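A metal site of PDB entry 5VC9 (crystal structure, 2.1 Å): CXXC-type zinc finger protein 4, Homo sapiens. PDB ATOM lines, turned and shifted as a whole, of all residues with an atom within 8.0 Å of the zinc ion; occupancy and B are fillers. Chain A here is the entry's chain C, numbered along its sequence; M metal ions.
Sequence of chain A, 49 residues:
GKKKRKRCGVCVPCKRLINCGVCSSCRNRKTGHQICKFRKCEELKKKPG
The guanidinium group of Arg 7 lies within hydrogen-bond range of the backbone carbonyl oxygen of Cys 14. N of Val 10 sits close to SG of Cys 8 (3.4 Å). The backbone NH (N) of Gly 9 sits close to the side-chain sulfur (SG) of Cys 14 (3.2 Å). N of Glu 43 sits close to SG of Cys 41, at 3.4 Å. The side-chain sulfur (SG) of Cys 11 lies close to the backbone NH (N) of Glu 42, at 3.5 Å.
N of Gly 9 touches the zinc ion, 3.7 Å away. Five residues have an atom within 4 Å of the zinc ion: Cys 8, Gly 9, Cys 11, Cys 14 and Cys 41.
The zinc ion is bound by SG of Cys 11 (2.3 Å), SG of Cys 8 (2.3 Å), SG of Cys 14 (2.3 Å) and SG of Cys 41 (2.3 Å). The zinc ion has four donor atoms within binding distance.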
ATOM      1  N   LYS A   6     -14.994   0.007  22.089  1.00  0.00           N
ATOM      2  CA  LYS A   6     -15.769  -1.274  22.173  1.00  0.00           C
ATOM      3  C   LYS A   6     -16.822  -1.307  21.056  1.00  0.00           C
ATOM      4  O   LYS A   6     -17.479  -0.313  20.794  1.00  0.00           O
ATOM      5  CB  LYS A   6     -16.512  -1.420  23.546  1.00  0.00           C
ATOM      6  CG  LYS A   6     -15.661  -1.170  24.813  1.00  0.00           C
ATOM      7  N   ARG A   7     -17.004  -2.474  20.441  1.00  0.00           N
ATOM      8  CA  ARG A   7     -18.137  -2.740  19.607  1.00  0.00           C
ATOM      9  C   ARG A   7     -19.463  -2.408  20.334  1.00  0.00           C
ATOM     10  O   ARG A   7     -19.514  -2.373  21.574  1.00  0.00           O
ATOM     11  CB  ARG A   7     -18.149  -4.204  19.173  1.00  0.00           C
ATOM     12  CG  ARG A   7     -18.399  -5.207  20.293  1.00  0.00           C
ATOM     13  CD  ARG A   7     -18.263  -6.639  19.814  1.00  0.00           C
ATOM     14  NE  ARG A   7     -18.815  -7.508  20.831  1.00  0.00           N
ATOM     15  CZ  ARG A   7     -19.902  -8.307  20.731  1.00  0.00           C
ATOM     16  NH1 ARG A   7     -20.288  -8.991  21.812  1.00  0.00           N
ATOM     17  NH2 ARG A   7     -20.570  -8.471  19.595  1.00  0.00           N
ATOM     18  N   CYS A   8     -20.513  -2.163  19.550  1.00  0.00           N
ATOM     19  CA  CYS A   8     -21.757  -1.736  20.113  1.00  0.00           C
ATOM     20  C   CYS A   8     -22.593  -2.921  20.589  1.00  0.00           C
ATOM     21  O   CYS A   8     -23.467  -2.749  21.447  1.00  0.00           O
ATOM     22  CB  CYS A   8     -22.542  -0.891  19.116  1.00  0.00           C
ATOM     23  SG  CYS A   8     -23.482  -1.848  17.960  1.00  0.00           S
ATOM     24  N   GLY A   9     -22.372  -4.115  20.003  1.00  0.00           N
ATOM     25  CA  GLY A   9     -23.047  -5.345  20.498  1.00  0.00           C
ATOM     26  C   GLY A   9     -24.497  -5.539  20.092  1.00  0.00           C
ATOM     27  O   GLY A   9     -25.084  -6.588  20.389  1.00  0.00           O
ATOM     28  N   VAL A  10     -25.075  -4.560  19.375  1.00  0.00           N
ATOM     29  CA  VAL A  10     -26.494  -4.585  18.989  1.00  0.00           C
ATOM     30  C   VAL A  10     -26.789  -4.485  17.485  1.00  0.00           C
ATOM     31  O   VAL A  10     -27.897  -4.837  17.079  1.00  0.00           O
ATOM     32  CB  VAL A  10     -27.297  -3.472  19.718  1.00  0.00           C
ATOM     33  CG1 VAL A  10     -27.356  -3.759  21.202  1.00  0.00           C
ATOM     34  CG2 VAL A  10     -26.715  -2.079  19.423  1.00  0.00           C
ATOM     35  N   CYS A  11     -25.824  -3.999  16.684  1.00  0.00           N
ATOM     36  CA  CYS A  11     -26.001  -3.921  15.239  1.00  0.00           C
ATOM     37  C   CYS A  11     -25.989  -5.348  14.633  1.00  0.00           C
ATOM     38  O   CYS A  11     -25.631  -6.305  15.302  1.00  0.00           O
ATOM     39  CB  CYS A  11     -24.943  -3.014  14.607  1.00  0.00           C
ATOM     40  SG  CYS A  11     -23.255  -3.677  14.569  1.00  0.00           S
ATOM     41  N   VAL A  12     -26.438  -5.494  13.382  1.00  0.00           N
ATOM     42  CA  VAL A  12     -26.503  -6.843  12.741  1.00  0.00           C
ATOM     43  C   VAL A  12     -25.110  -7.487  12.719  1.00  0.00           C
ATOM     44  O   VAL A  12     -24.960  -8.604  13.199  1.00  0.00           O
ATOM     45  CB  VAL A  12     -27.188  -6.789  11.332  1.00  0.00           C
ATOM     46  CG1 VAL A  12     -26.931  -8.079  10.492  1.00  0.00           C
ATOM     47  CG2 VAL A  12     -28.684  -6.520  11.506  1.00  0.00           C
ATOM     48  N   PRO A  13     -24.061  -6.751  12.232  1.00  0.00           N
ATOM     49  CA  PRO A  13     -22.713  -7.337  12.292  1.00  0.00           C
ATOM     50  C   PRO A  13     -22.293  -7.816  13.662  1.00  0.00           C
ATOM     51  O   PRO A  13     -21.748  -8.928  13.771  1.00  0.00           O
ATOM     52  CB  PRO A  13     -21.790  -6.201  11.762  1.00  0.00           C
ATOM     53  CG  PRO A  13     -22.689  -5.402  10.823  1.00  0.00           C
ATOM     54  CD  PRO A  13     -24.114  -5.558  11.328  1.00  0.00           C
ATOM     55  N   CYS A  14     -22.520  -7.001  14.702  1.00  0.00           N
ATOM     56  CA  CYS A  14     -22.146  -7.379  16.053  1.00  0.00           C
ATOM     57  C   CYS A  14     -22.849  -8.686  16.503  1.00  0.00           C
ATOM     58  O   CYS A  14     -22.234  -9.488  17.213  1.00  0.00           O
ATOM     59  CB  CYS A  14     -22.399  -6.241  17.046  1.00  0.00           C
ATOM     60  SG  CYS A  14     -21.116  -4.985  17.170  1.00  0.00           S
ATOM     61  N   LYS A  15     -24.095  -8.897  16.059  1.00  0.00           N
ATOM     62  CA  LYS A  15     -24.854 -10.128  16.412  1.00  0.00           C
ATOM     63  C   LYS A  15     -24.362 -11.429  15.634  1.00  0.00           C
ATOM     64  O   LYS A  15     -24.699 -12.555  16.038  1.00  0.00           O
ATOM     65  CB  LYS A  15     -26.380  -9.902  16.255  1.00  0.00           C
ATOM     66  CG  LYS A  15     -26.945  -8.900  17.320  1.00  0.00           C
ATOM     67  CD  LYS A  15     -28.474  -8.751  17.307  1.00  0.00           C
ATOM     68  N   ARG A  39     -18.825  -8.830  10.201  1.00  0.00           N
ATOM     69  CA  ARG A  39     -18.974  -8.708  11.692  1.00  0.00           C
ATOM     70  C   ARG A  39     -18.521  -7.373  12.197  1.00  0.00           C
ATOM     71  O   ARG A  39     -18.801  -7.030  13.357  1.00  0.00           O
ATOM     72  CB  ARG A  39     -18.183  -9.776  12.405  1.00  0.00           C
ATOM     73  CG  ARG A  39     -18.672 -11.171  12.094  1.00  0.00           C
ATOM     74  CD  ARG A  39     -17.837 -12.171  12.814  1.00  0.00           C
ATOM     75  NE  ARG A  39     -17.849 -11.961  14.274  1.00  0.00           N
ATOM     76  CZ  ARG A  39     -16.759 -11.956  15.073  1.00  0.00           C
ATOM     77  NH1 ARG A  39     -15.542 -12.186  14.585  1.00  0.00           N
ATOM     78  NH2 ARG A  39     -16.893 -11.779  16.403  1.00  0.00           N
ATOM     79  N   LYS A  40     -17.844  -6.599  11.349  1.00  0.00           N
ATOM     80  CA  LYS A  40     -17.333  -5.279  11.727  1.00  0.00           C
ATOM     81  C   LYS A  40     -18.482  -4.386  12.245  1.00  0.00           C
ATOM     82  O   LYS A  40     -19.486  -4.154  11.567  1.00  0.00           O
ATOM     83  CB  LYS A  40     -16.648  -4.612  10.554  1.00  0.00           C
ATOM     84  CG  LYS A  40     -16.111  -3.249  10.883  1.00  0.00           C
ATOM     85  CD  LYS A  40     -14.902  -3.351  11.816  1.00  0.00           C
ATOM     86  CE  LYS A  40     -14.061  -2.108  11.699  1.00  0.00           C
ATOM     87  NZ  LYS A  40     -13.008  -2.117  12.689  1.00  0.00           N
ATOM     88  N   CYS A  41     -18.333  -3.882  13.453  1.00  0.00           N
ATOM     89  CA  CYS A  41     -19.431  -3.053  14.071  1.00  0.00           C
ATOM     90  C   CYS A  41     -19.706  -1.807  13.227  1.00  0.00           C
ATOM     91  O   CYS A  41     -18.777  -1.012  12.947  1.00  0.00           O
ATOM     92  CB  CYS A  41     -19.101  -2.654  15.519  1.00  0.00           C
ATOM     93  SG  CYS A  41     -20.334  -1.575  16.253  1.00  0.00           S
ATOM     94  N   GLU A  42     -20.962  -1.593  12.860  1.00  0.00           N
ATOM     95  CA  GLU A  42     -21.340  -0.387  12.063  1.00  0.00           C
ATOM     96  C   GLU A  42     -20.847   0.899  12.691  1.00  0.00           C
ATOM     97  O   GLU A  42     -20.485   1.824  11.962  1.00  0.00           O
ATOM     98  CB  GLU A  42     -22.858  -0.239  11.855  1.00  0.00           C
ATOM     99  CG  GLU A  42     -23.588  -1.390  11.193  1.00  0.00           C
ATOM    100  CD  GLU A  42     -23.153  -1.689   9.758  1.00  0.00           C
ATOM    101  OE1 GLU A  42     -22.135  -1.121   9.251  1.00  0.00           O
ATOM    102  OE2 GLU A  42     -23.859  -2.496   9.112  1.00  0.00           O
ATOM    103  N   GLU A  43     -20.846   0.957  14.018  1.00  0.00           N
ATOM    104  CA  GLU A  43     -20.419   2.176  14.740  1.00  0.00           C
ATOM    105  C   GLU A  43     -18.908   2.343  14.789  1.00  0.00           C
ATOM    106  O   GLU A  43     -18.434   3.383  15.234  1.00  0.00           O
ATOM    107  CB  GLU A  43     -20.969   2.215  16.191  1.00  0.00           C
ATOM    108  CG  GLU A  43     -22.460   1.955  16.332  1.00  0.00           C
ATOM    109  CD  GLU A  43     -23.307   2.926  15.509  1.00  0.00           C
ATOM    110  OE1 GLU A  43     -22.915   4.117  15.373  1.00  0.00           O
ATOM    111  OE2 GLU A  43     -24.370   2.495  15.008  1.00  0.00           O
ATOM    112  N   LEU A  44     -18.153   1.321  14.385  1.00  0.00           N
ATOM    113  CA  LEU A  44     -16.684   1.457  14.392  1.00  0.00           C
ATOM    114  C   LEU A  44     -16.078   1.760  13.025  1.00  0.00           C
ATOM    115  O   LEU A  44     -14.885   1.919  12.917  1.00  0.00           O
ATOM    116  CB  LEU A  44     -16.065   0.231  15.008  1.00  0.00           C
ATOM    117  CG  LEU A  44     -16.515  -0.062  16.425  1.00  0.00           C
ATOM    118  CD1 LEU A  44     -15.835  -1.348  16.879  1.00  0.00           C
ATOM    119  CD2 LEU A  44     -16.227   1.077  17.437  1.00  0.00           C
HETATM  120 ZN    ZN M   1     -22.161  -3.029  16.460  1.00  0.00          ZN
